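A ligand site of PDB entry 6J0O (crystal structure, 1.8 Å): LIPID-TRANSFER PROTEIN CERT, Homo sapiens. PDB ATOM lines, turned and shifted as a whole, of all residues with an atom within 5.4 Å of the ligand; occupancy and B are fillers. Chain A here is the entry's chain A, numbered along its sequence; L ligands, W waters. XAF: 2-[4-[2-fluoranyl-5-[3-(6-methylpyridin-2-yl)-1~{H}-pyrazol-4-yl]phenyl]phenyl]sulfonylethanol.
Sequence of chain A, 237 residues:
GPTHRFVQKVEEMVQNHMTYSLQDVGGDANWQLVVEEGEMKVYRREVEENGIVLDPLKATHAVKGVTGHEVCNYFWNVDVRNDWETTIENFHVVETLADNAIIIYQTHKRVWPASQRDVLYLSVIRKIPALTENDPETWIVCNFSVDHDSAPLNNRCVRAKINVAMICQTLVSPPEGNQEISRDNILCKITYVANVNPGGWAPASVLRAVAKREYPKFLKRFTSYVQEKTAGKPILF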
ATOM      1  N   PHE A  75      -3.996 -11.114   1.949  1.00  0.00           N
ATOM      2  CA  PHE A  75      -3.118 -10.612   0.872  1.00  0.00           C
ATOM      3  C   PHE A  75      -3.807  -9.566  -0.003  1.00  0.00           C
ATOM      4  O   PHE A  75      -3.148  -8.637  -0.518  1.00  0.00           O
ATOM      5  CB  PHE A  75      -2.649 -11.807   0.005  1.00  0.00           C
ATOM      6  CG  PHE A  75      -1.576 -11.454  -1.020  1.00  0.00           C
ATOM      7  CD1 PHE A  75      -0.306 -11.054  -0.620  1.00  0.00           C
ATOM      8  CD2 PHE A  75      -1.812 -11.623  -2.382  1.00  0.00           C
ATOM      9  CE1 PHE A  75       0.711 -10.780  -1.549  1.00  0.00           C
ATOM     10  CE2 PHE A  75      -0.798 -11.347  -3.297  1.00  0.00           C
ATOM     11  CZ  PHE A  75       0.454 -10.940  -2.887  1.00  0.00           C
ATOM     12  N   ARG A  81      -2.613  -3.837   4.488  1.00  0.00           N
ATOM     13  CA  ARG A  81      -1.403  -3.872   3.702  1.00  0.00           C
ATOM     14  C   ARG A  81      -0.204  -3.423   4.532  1.00  0.00           C
ATOM     15  O   ARG A  81       0.817  -4.096   4.534  1.00  0.00           O
ATOM     16  CB  ARG A  81      -1.600  -3.064   2.410  1.00  0.00           C
ATOM     17  CG  ARG A  81      -0.564  -3.326   1.323  1.00  0.00           C
ATOM     18  CD  ARG A  81      -0.737  -4.670   0.633  1.00  0.00           C
ATOM     19  NE  ARG A  81      -1.067  -4.394  -0.751  1.00  0.00           N
ATOM     20  CZ  ARG A  81      -2.169  -4.806  -1.330  1.00  0.00           C
ATOM     21  NH1 ARG A  81      -2.364  -4.511  -2.598  1.00  0.00           N
ATOM     22  NH2 ARG A  81      -3.044  -5.545  -0.636  1.00  0.00           N
ATOM     23  N   TRP A  84       1.895  -5.683   7.013  1.00  0.00           N
ATOM     24  CA  TRP A  84       2.846  -6.712   6.615  1.00  0.00           C
ATOM     25  C   TRP A  84       3.840  -6.243   5.535  1.00  0.00           C
ATOM     26  O   TRP A  84       4.917  -6.828   5.424  1.00  0.00           O
ATOM     27  CB  TRP A  84       2.153  -8.049   6.236  1.00  0.00           C
ATOM     28  CG  TRP A  84       1.201  -7.959   5.081  1.00  0.00           C
ATOM     29  CD1 TRP A  84      -0.154  -7.788   5.143  1.00  0.00           C
ATOM     30  CD2 TRP A  84       1.527  -8.047   3.678  1.00  0.00           C
ATOM     31  NE1 TRP A  84      -0.705  -7.770   3.876  1.00  0.00           N
ATOM     32  CE2 TRP A  84       0.315  -7.883   2.959  1.00  0.00           C
ATOM     33  CE3 TRP A  84       2.720  -8.207   2.967  1.00  0.00           C
ATOM     34  CZ2 TRP A  84       0.287  -7.886   1.565  1.00  0.00           C
ATOM     35  CZ3 TRP A  84       2.702  -8.182   1.592  1.00  0.00           C
ATOM     36  CH2 TRP A  84       1.488  -8.046   0.899  1.00  0.00           C
ATOM     37  N   GLU A  85       3.456  -5.288   4.687  1.00  0.00           N
ATOM     38  CA  GLU A  85       4.360  -4.790   3.659  1.00  0.00           C
ATOM     39  C   GLU A  85       5.501  -4.017   4.296  1.00  0.00           C
ATOM     40  O   GLU A  85       5.261  -3.307   5.274  1.00  0.00           O
ATOM     41  CB  GLU A  85       3.671  -3.715   2.824  1.00  0.00           C
ATOM     42  CG  GLU A  85       2.734  -4.280   1.805  1.00  0.00           C
ATOM     43  CD  GLU A  85       3.343  -4.588   0.445  1.00  0.00           C
ATOM     44  OE1 GLU A  85       2.639  -4.421  -0.568  1.00  0.00           O
ATOM     45  OE2 GLU A  85       4.504  -4.987   0.406  1.00  0.00           O
ATOM     46  N   THR A  87       8.167  -2.741   1.805  1.00  0.00           N
ATOM     47  CA  THR A  87       8.915  -2.008   0.791  1.00  0.00           C
ATOM     48  C   THR A  87       8.087  -0.893   0.128  1.00  0.00           C
ATOM     49  O   THR A  87       8.590  -0.198  -0.750  1.00  0.00           O
ATOM     50  CB  THR A  87       9.456  -2.954  -0.291  1.00  0.00           C
ATOM     51  OG1 THR A  87       8.360  -3.431  -1.091  1.00  0.00           O
ATOM     52  CG2 THR A  87      10.235  -4.112   0.282  1.00  0.00           C
ATOM     53  N   ILE A  88       6.826  -0.734   0.514  1.00  0.00           N
ATOM     54  CA  ILE A  88       5.946   0.276  -0.083  1.00  0.00           C
ATOM     55  C   ILE A  88       6.241   1.654   0.507  1.00  0.00           C
ATOM     56  O   ILE A  88       6.395   1.813   1.725  1.00  0.00           O
ATOM     57  CB  ILE A  88       4.463  -0.122   0.154  1.00  0.00           C
ATOM     58  CG1 ILE A  88       4.077  -1.414  -0.561  1.00  0.00           C
ATOM     59  CG2 ILE A  88       3.508   1.026  -0.137  1.00  0.00           C
ATOM     60  CD1 ILE A  88       4.142  -1.345  -2.037  1.00  0.00           C
ATOM     61  N   GLN A 106       1.160   2.074  -6.768  1.00  0.00           N
ATOM     62  CA  GLN A 106       2.034   2.143  -5.609  1.00  0.00           C
ATOM     63  C   GLN A 106       3.474   2.440  -6.021  1.00  0.00           C
ATOM     64  O   GLN A 106       3.860   2.233  -7.162  1.00  0.00           O
ATOM     65  CB  GLN A 106       1.938   0.884  -4.728  1.00  0.00           C
ATOM     66  CG  GLN A 106       2.467  -0.372  -5.406  1.00  0.00           C
ATOM     67  CD  GLN A 106       2.126  -1.665  -4.673  1.00  0.00           C
ATOM     68  OE1 GLN A 106       1.067  -1.799  -4.080  1.00  0.00           O
ATOM     69  NE2 GLN A 106       3.023  -2.638  -4.733  1.00  0.00           N
ATOM     70  N   HIS A 108       7.585   1.980  -4.546  1.00  0.00           N
ATOM     71  CA  HIS A 108       8.433   1.178  -3.675  1.00  0.00           C
ATOM     72  C   HIS A 108       9.679   1.960  -3.231  1.00  0.00           C
ATOM     73  O   HIS A 108      10.163   2.858  -3.919  1.00  0.00           O
ATOM     74  CB  HIS A 108       8.878  -0.108  -4.385  1.00  0.00           C
ATOM     75  CG  HIS A 108       7.737  -1.067  -4.549  1.00  0.00           C
ATOM     76  ND1 HIS A 108       7.429  -2.007  -3.582  1.00  0.00           N
ATOM     77  CD2 HIS A 108       6.769  -1.147  -5.483  1.00  0.00           C
ATOM     78  CE1 HIS A 108       6.369  -2.686  -3.979  1.00  0.00           C
ATOM     79  NE2 HIS A 108       5.928  -2.154  -5.104  1.00  0.00           N
ATOM     80  N   LYS A 109      10.192   1.571  -2.072  1.00  0.00           N
ATOM     81  CA  LYS A 109      11.501   2.000  -1.582  1.00  0.00           C
ATOM     82  C   LYS A 109      12.602   1.746  -2.615  1.00  0.00           C
ATOM     83  O   LYS A 109      12.647   0.709  -3.285  1.00  0.00           O
ATOM     84  CB  LYS A 109      11.795   1.346  -0.239  1.00  0.00           C
ATOM     85  CG  LYS A 109      10.891   1.908   0.853  1.00  0.00           C
ATOM     86  CD  LYS A 109      11.075   1.268   2.203  1.00  0.00           C
ATOM     87  CE  LYS A 109       9.848   1.420   3.069  1.00  0.00           C
ATOM     88  NZ  LYS A 109      10.019   0.664   4.334  1.00  0.00           N
ATOM     89  N   ARG A 110      13.489   2.736  -2.735  1.00  0.00           N
ATOM     90  CA  ARG A 110      14.516   2.645  -3.756  1.00  0.00           C
ATOM     91  C   ARG A 110      15.473   1.472  -3.483  1.00  0.00           C
ATOM     92  O   ARG A 110      15.795   1.199  -2.326  1.00  0.00           O
ATOM     93  CB  ARG A 110      15.197   4.015  -3.807  1.00  0.00           C
ATOM     94  CG  ARG A 110      16.261   4.124  -4.883  1.00  0.00           C
ATOM     95  CD  ARG A 110      16.693   5.582  -5.000  1.00  0.00           C
ATOM     96  NE  ARG A 110      17.762   5.554  -5.973  1.00  0.00           N
ATOM     97  CZ  ARG A 110      19.055   5.460  -5.686  1.00  0.00           C
ATOM     98  NH1 ARG A 110      19.456   5.422  -4.422  1.00  0.00           N
ATOM     99  NH2 ARG A 110      19.937   5.442  -6.673  1.00  0.00           N
ATOM    100  N   VAL A 111      15.868   0.719  -4.513  1.00  0.00           N
ATOM    101  CA  VAL A 111      16.980  -0.240  -4.435  1.00  0.00           C
ATOM    102  C   VAL A 111      18.236   0.379  -5.091  1.00  0.00           C
ATOM    103  O   VAL A 111      18.361   0.307  -6.308  1.00  0.00           O
ATOM    104  CB  VAL A 111      16.572  -1.580  -5.102  1.00  0.00           C
ATOM    105  CG1 VAL A 111      17.696  -2.638  -5.159  1.00  0.00           C
ATOM    106  CG2 VAL A 111      15.347  -2.178  -4.386  1.00  0.00           C
ATOM    107  N   ARG A 117      10.994   2.459  -8.179  1.00  0.00           N
ATOM    108  CA  ARG A 117       9.991   1.882  -9.069  1.00  0.00           C
ATOM    109  C   ARG A 117       8.581   2.207  -8.555  1.00  0.00           C
ATOM    110  O   ARG A 117       8.340   2.195  -7.338  1.00  0.00           O
ATOM    111  CB  ARG A 117      10.122   0.339  -9.134  1.00  0.00           C
ATOM    112  CG  ARG A 117      10.932  -0.186 -10.329  1.00  0.00           C
ATOM    113  CD  ARG A 117      12.293   0.510 -10.498  1.00  0.00           C
ATOM    114  NE  ARG A 117      12.891  -0.009 -11.740  1.00  0.00           N
ATOM    115  CZ  ARG A 117      14.039   0.387 -12.256  1.00  0.00           C
ATOM    116  NH1 ARG A 117      14.754   1.317 -11.627  1.00  0.00           N
ATOM    117  NH2 ARG A 117      14.473  -0.124 -13.398  1.00  0.00           N
ATOM    118  N   VAL A 119       4.237   1.094  -9.814  1.00  0.00           N
ATOM    119  CA  VAL A 119       3.552   0.007 -10.478  1.00  0.00           C
ATOM    120  C   VAL A 119       2.046   0.313 -10.430  1.00  0.00           C
ATOM    121  O   VAL A 119       1.583   1.052  -9.577  1.00  0.00           O
ATOM    122  CB  VAL A 119       3.865  -1.339  -9.785  1.00  0.00           C
ATOM    123  CG1 VAL A 119       3.391  -1.361  -8.362  1.00  0.00           C
ATOM    124  CG2 VAL A 119       3.303  -2.549 -10.538  1.00  0.00           C
ATOM    125  N   TYR A 121      -1.524  -1.746 -11.107  1.00  0.00           N
ATOM    126  CA  TYR A 121      -1.952  -3.095 -11.384  1.00  0.00           C
ATOM    127  C   TYR A 121      -3.404  -3.330 -10.963  1.00  0.00           C
ATOM    128  O   TYR A 121      -3.908  -2.712 -10.032  1.00  0.00           O
ATOM    129  CB  TYR A 121      -1.068  -4.128 -10.651  1.00  0.00           C
ATOM    130  CG  TYR A 121      -0.954  -3.992  -9.139  1.00  0.00           C
ATOM    131  CD1 TYR A 121      -0.118  -3.055  -8.533  1.00  0.00           C
ATOM    132  CD2 TYR A 121      -1.657  -4.844  -8.302  1.00  0.00           C
ATOM    133  CE1 TYR A 121       0.031  -2.978  -7.150  1.00  0.00           C
ATOM    134  CE2 TYR A 121      -1.524  -4.763  -6.923  1.00  0.00           C
ATOM    135  CZ  TYR A 121      -0.668  -3.858  -6.344  1.00  0.00           C
ATOM    136  OH  TYR A 121      -0.593  -3.744  -4.988  1.00  0.00           O
ATOM    137  N   ASN A 143      -2.296 -10.290  -9.179  1.00  0.00           N
ATOM    138  CA  ASN A 143      -1.968  -8.866  -9.274  1.00  0.00           C
ATOM    139  C   ASN A 143      -1.243  -8.681 -10.604  1.00  0.00           C
ATOM    140  O   ASN A 143      -0.128  -9.194 -10.771  1.00  0.00           O
ATOM    141  CB  ASN A 143      -1.087  -8.374  -8.122  1.00  0.00           C
ATOM    142  CG  ASN A 143      -1.788  -8.377  -6.765  1.00  0.00           C
ATOM    143  OD1 ASN A 143      -3.010  -8.239  -6.682  1.00  0.00           O
ATOM    144  ND2 ASN A 143      -1.051  -8.539  -5.674  1.00  0.00           N
ATOM    145  N   ALA A 160       7.546  -0.358 -13.245  1.00  0.00           N
ATOM    146  CA  ALA A 160       7.691  -1.809 -13.343  1.00  0.00           C
ATOM    147  C   ALA A 160       6.396  -2.382 -13.887  1.00  0.00           C
ATOM    148  O   ALA A 160       5.351  -1.742 -13.757  1.00  0.00           O
ATOM    149  CB  ALA A 160       7.972  -2.401 -11.990  1.00  0.00           C
ATOM    150  N   ILE A 162       4.165  -6.059 -13.532  1.00  0.00           N
ATOM    151  CA  ILE A 162       4.099  -7.283 -12.723  1.00  0.00           C
ATOM    152  C   ILE A 162       3.037  -8.259 -13.219  1.00  0.00           C
ATOM    153  O   ILE A 162       2.003  -7.903 -13.805  1.00  0.00           O
ATOM    154  CB  ILE A 162       3.956  -6.977 -11.226  1.00  0.00           C
ATOM    155  CG1 ILE A 162       2.557  -6.434 -10.847  1.00  0.00           C
ATOM    156  CG2 ILE A 162       5.091  -6.018 -10.802  1.00  0.00           C
ATOM    157  CD1 ILE A 162       2.303  -6.313  -9.327  1.00  0.00           C
ATOM    158  N   VAL A 164       1.784 -11.335 -10.664  1.00  0.00           N
ATOM    159  CA  VAL A 164       1.974 -12.056  -9.402  1.00  0.00           C
ATOM    160  C   VAL A 164       0.693 -12.837  -9.088  1.00  0.00           C
ATOM    161  O   VAL A 164      -0.443 -12.373  -9.325  1.00  0.00           O
ATOM    162  CB  VAL A 164       2.313 -11.069  -8.261  1.00  0.00           C
ATOM    163  CG1 VAL A 164       2.305 -11.710  -6.865  1.00  0.00           C
ATOM    164  CG2 VAL A 164       3.653 -10.355  -8.473  1.00  0.00           C
ATOM    165  N   TYR A 192       3.322 -19.243  -4.672  1.00  0.00           N
ATOM    166  CA  TYR A 192       3.442 -17.818  -4.943  1.00  0.00           C
ATOM    167  C   TYR A 192       4.345 -17.649  -6.173  1.00  0.00           C
ATOM    168  O   TYR A 192       5.447 -18.216  -6.232  1.00  0.00           O
ATOM    169  CB  TYR A 192       4.062 -17.122  -3.741  1.00  0.00           C
ATOM    170  CG  TYR A 192       4.424 -15.675  -3.971  1.00  0.00           C
ATOM    171  CD1 TYR A 192       3.463 -14.695  -3.895  1.00  0.00           C
ATOM    172  CD2 TYR A 192       5.718 -15.298  -4.364  1.00  0.00           C
ATOM    173  CE1 TYR A 192       3.794 -13.350  -4.114  1.00  0.00           C
ATOM    174  CE2 TYR A 192       6.042 -13.971  -4.662  1.00  0.00           C
ATOM    175  CZ  TYR A 192       5.083 -12.990  -4.483  1.00  0.00           C
ATOM    176  OH  TYR A 192       5.400 -11.678  -4.744  1.00  0.00           O
ATOM    177  N   VAL A 196       8.303 -10.116 -12.497  1.00  0.00           N
ATOM    178  CA  VAL A 196       8.478  -8.685 -12.358  1.00  0.00           C
ATOM    179  C   VAL A 196       9.383  -8.197 -13.487  1.00  0.00           C
ATOM    180  O   VAL A 196      10.512  -8.677 -13.664  1.00  0.00           O
ATOM    181  CB  VAL A 196       8.974  -8.286 -10.950  1.00  0.00           C
ATOM    182  CG1 VAL A 196       9.284  -6.786 -10.856  1.00  0.00           C
ATOM    183  CG2 VAL A 196       7.993  -8.668  -9.823  1.00  0.00           C
ATOM    184  N   VAL A 210      18.829  -8.886  -3.949  1.00  0.00           N
ATOM    185  CA  VAL A 210      17.615  -8.406  -3.301  1.00  0.00           C
ATOM    186  C   VAL A 210      16.477  -9.412  -3.435  1.00  0.00           C
ATOM    187  O   VAL A 210      15.752  -9.639  -2.461  1.00  0.00           O
ATOM    188  CB  VAL A 210      17.243  -7.026  -3.850  1.00  0.00           C
ATOM    189  CG1 VAL A 210      15.890  -6.548  -3.387  1.00  0.00           C
ATOM    190  CG2 VAL A 210      18.335  -6.032  -3.461  1.00  0.00           C
ATOM    191  N   ALA A 211      16.315 -10.067  -4.589  1.00  0.00           N
ATOM    192  CA  ALA A 211      15.236 -11.032  -4.704  1.00  0.00           C
ATOM    193  C   ALA A 211      15.496 -12.160  -3.713  1.00  0.00           C
ATOM    194  O   ALA A 211      14.578 -12.665  -3.057  1.00  0.00           O
ATOM    195  CB  ALA A 211      15.062 -11.519  -6.149  1.00  0.00           C
ATOM    196  N   GLU A 214      14.805 -10.816  -0.124  1.00  0.00           N
ATOM    197  CA  GLU A 214      13.549 -10.195   0.239  1.00  0.00           C
ATOM    198  C   GLU A 214      12.357 -11.136   0.027  1.00  0.00           C
ATOM    199  O   GLU A 214      11.353 -11.046   0.762  1.00  0.00           O
ATOM    200  CB  GLU A 214      13.263  -8.939  -0.566  1.00  0.00           C
ATOM    201  CG  GLU A 214      14.171  -7.775  -0.179  1.00  0.00           C
ATOM    202  CD  GLU A 214      13.954  -7.263   1.235  1.00  0.00           C
ATOM    203  OE1 GLU A 214      12.764  -7.042   1.624  1.00  0.00           O
ATOM    204  OE2 GLU A 214      14.980  -7.100   1.941  1.00  0.00           O
ATOM    205  N   TYR A 215      12.405 -11.974  -1.009  1.00  0.00           N
ATOM    206  CA  TYR A 215      11.230 -12.811  -1.249  1.00  0.00           C
ATOM    207  C   TYR A 215      10.984 -13.738  -0.047  1.00  0.00           C
ATOM    208  O   TYR A 215       9.841 -13.902   0.411  1.00  0.00           O
ATOM    209  CB  TYR A 215      11.285 -13.525  -2.609  1.00  0.00           C
ATOM    210  CG  TYR A 215      10.821 -12.724  -3.788  1.00  0.00           C
ATOM    211  CD1 TYR A 215       9.487 -12.381  -3.940  1.00  0.00           C
ATOM    212  CD2 TYR A 215      11.711 -12.304  -4.763  1.00  0.00           C
ATOM    213  CE1 TYR A 215       9.029 -11.679  -5.045  1.00  0.00           C
ATOM    214  CE2 TYR A 215      11.282 -11.597  -5.878  1.00  0.00           C
ATOM    215  CZ  TYR A 215       9.937 -11.252  -6.010  1.00  0.00           C
ATOM    216  OH  TYR A 215       9.490 -10.544  -7.099  1.00  0.00           O
ATOM    217  N   PHE A 218       9.607 -11.674   2.873  1.00  0.00           N
ATOM    218  CA  PHE A 218       8.202 -11.349   2.624  1.00  0.00           C
ATOM    219  C   PHE A 218       7.304 -12.563   2.945  1.00  0.00           C
ATOM    220  O   PHE A 218       6.276 -12.425   3.638  1.00  0.00           O
ATOM    221  CB  PHE A 218       7.966 -10.756   1.213  1.00  0.00           C
ATOM    222  CG  PHE A 218       6.632 -11.152   0.612  1.00  0.00           C
ATOM    223  CD1 PHE A 218       5.427 -10.790   1.187  1.00  0.00           C
ATOM    224  CD2 PHE A 218       6.578 -12.034  -0.450  1.00  0.00           C
ATOM    225  CE1 PHE A 218       4.213 -11.215   0.641  1.00  0.00           C
ATOM    226  CE2 PHE A 218       5.373 -12.487  -0.990  1.00  0.00           C
ATOM    227  CZ  PHE A 218       4.172 -12.086  -0.435  1.00  0.00           C
HETATM  228  F1  XAF L   1       6.963  -4.289  -8.424  1.00  0.00           F
HETATM  229  C9  XAF L   1       7.928  -4.171  -7.504  1.00  0.00           C
HETATM  230  C8  XAF L   1       9.063  -3.338  -7.736  1.00  0.00           C
HETATM  231  C10 XAF L   1       7.829  -4.890  -6.309  1.00  0.00           C
HETATM  232  C11 XAF L   1       8.820  -4.717  -5.312  1.00  0.00           C
HETATM  233  C12 XAF L   1      10.003  -3.915  -5.502  1.00  0.00           C
HETATM  234  C15 XAF L   1      10.982  -3.746  -4.405  1.00  0.00           C
HETATM  235  C17 XAF L   1      11.479  -4.702  -3.457  1.00  0.00           C
HETATM  236  C21 XAF L   1      11.237  -6.174  -3.455  1.00  0.00           C
HETATM  237  C20 XAF L   1      12.193  -7.010  -4.101  1.00  0.00           C
HETATM  238  C19 XAF L   1      12.022  -8.398  -4.144  1.00  0.00           C
HETATM  239  N3  XAF L   1      10.142  -6.679  -2.868  1.00  0.00           N
HETATM  240  C22 XAF L   1       9.979  -8.029  -2.893  1.00  0.00           C
HETATM  241  C23 XAF L   1       8.753  -8.605  -2.224  1.00  0.00           C
HETATM  242  C18 XAF L   1      10.871  -8.888  -3.511  1.00  0.00           C
HETATM  243  N2  XAF L   1      12.302  -4.122  -2.570  1.00  0.00           N
HETATM  244  N1  XAF L   1      12.325  -2.789  -2.851  1.00  0.00           N
HETATM  245  C16 XAF L   1      11.538  -2.550  -3.964  1.00  0.00           C
HETATM  246  C7  XAF L   1      10.051  -3.207  -6.733  1.00  0.00           C
HETATM  247  C1  XAF L   1       6.609  -5.742  -6.009  1.00  0.00           C
HETATM  248  C6  XAF L   1       5.273  -5.348  -6.373  1.00  0.00           C
HETATM  249  C5  XAF L   1       4.172  -6.177  -5.961  1.00  0.00           C
HETATM  250  C4  XAF L   1       4.445  -7.304  -5.236  1.00  0.00           C
HETATM  251  C3  XAF L   1       5.725  -7.727  -4.835  1.00  0.00           C
HETATM  252  C2  XAF L   1       6.813  -6.880  -5.194  1.00  0.00           C
HETATM  253  S1  XAF L   1       3.031  -8.279  -4.712  1.00  0.00           S
HETATM  254  O1  XAF L   1       2.105  -8.039  -5.792  1.00  0.00           O
HETATM  255  O2  XAF L   1       3.534  -9.603  -4.264  1.00  0.00           O
HETATM  256  C13 XAF L   1       2.404  -7.548  -3.124  1.00  0.00           C
HETATM  257  C14 XAF L   1       1.728  -6.171  -3.343  1.00  0.00           C
HETATM  258  O3  XAF L   1       2.764  -5.194  -3.216  1.00  0.00           O
HETATM  259  O   HOH W   1       5.324  -5.592  -2.193  1.00  0.00           O
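Water W1 lies within hydrogen-bond range of an oxygen (O3) of the ligand (2.8 Å) and the side-chain carboxylate (OE2) of Glu 85 (2.8 Å).
CZ of Phe 75 touches O2 of the ligand, 3.6 Å away.
Thr 87 touches the ligand.
His 108 touches the ligand (CE1 to C11, 3.5 Å).
Lys 109 touches the ligand (O to C16, 3.5 Å).
Val 111 touches the ligand (CG2 to N1, 3.4 Å).
Tyr 121 touches the ligand (OH to C14, 3.7 Å).
Ile 162 touches the ligand (CG2 to F1, 3.5 Å).
Val 164 touches the ligand.
CG1 of Val 210 touches C20 of the ligand, at 3.8 Å.
Glu 214 touches the ligand.
Tyr 215 touches the ligand.
Hydrophobic or aromatic side chains within 4 Å of the ligand: Phe 75, His 108, Val 111, Ile 162, Val 164, Tyr 192, Val 210 and Tyr 215.
Within 4 Å of the ligand: Phe 75, Glu 85, Thr 87, Gln 106, His 108, Lys 109, Val 111, Tyr 121, Asn 143, Ile 162, Val 164, Tyr 192, Val 210, Glu 214 and Tyr 215.
Along chain A the residues within 4 Å of the ligand span positions 75 to 215.
The side-chain carboxylate of Glu 85 lies within salt-bridge range of the guanidinium group of Arg 81 (3.7 Å).
The side-chain amide nitrogen (NE2) of Gln 106 sits at hydrogen-bond distance from a ring nitrogen (NE2) of His 108 (3.0 Å).
The side-chain amide oxygen (OE1) of Gln 106 sits at hydrogen-bond distance from the side-chain hydroxyl (OH) of Tyr 121, 2.7 Å away.
N of Val 119 sits at hydrogen-bond distance from O of Gln 106 (2.9 Å).
The backbone NH of Asn 143 sits at hydrogen-bond distance from the backbone carbonyl oxygen of Val 164, 2.8 Å away.
A ring nitrogen (ND1) of His 108 is in hydrogen-bond range of the side-chain hydroxyl of Thr 87 (3.0 Å).
The backbone NH (N) of His 108 sits at hydrogen-bond distance from the backbone carbonyl oxygen (O) of Arg 117 (2.9 Å).
The guanidinium group (NH2) of Arg 81 sits at hydrogen-bond distance from the backbone carbonyl oxygen (O) of Phe 75 (3.1 Å).
The side-chain carboxylate of Glu 85 sits at hydrogen-bond distance from an oxygen (O3) of the ligand, 2.8 Å away.
An oxygen (O2) of the ligand is in hydrogen-bond range of the side-chain hydroxyl of Tyr 192, at 2.8 Å.
O3 of the ligand sits at hydrogen-bond distance from NE2 of Gln 106 (3.0 Å).
An oxygen (O1) of the ligand lies within hydrogen-bond range of the side-chain amide nitrogen (ND2) of Asn 143 (3.2 Å).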
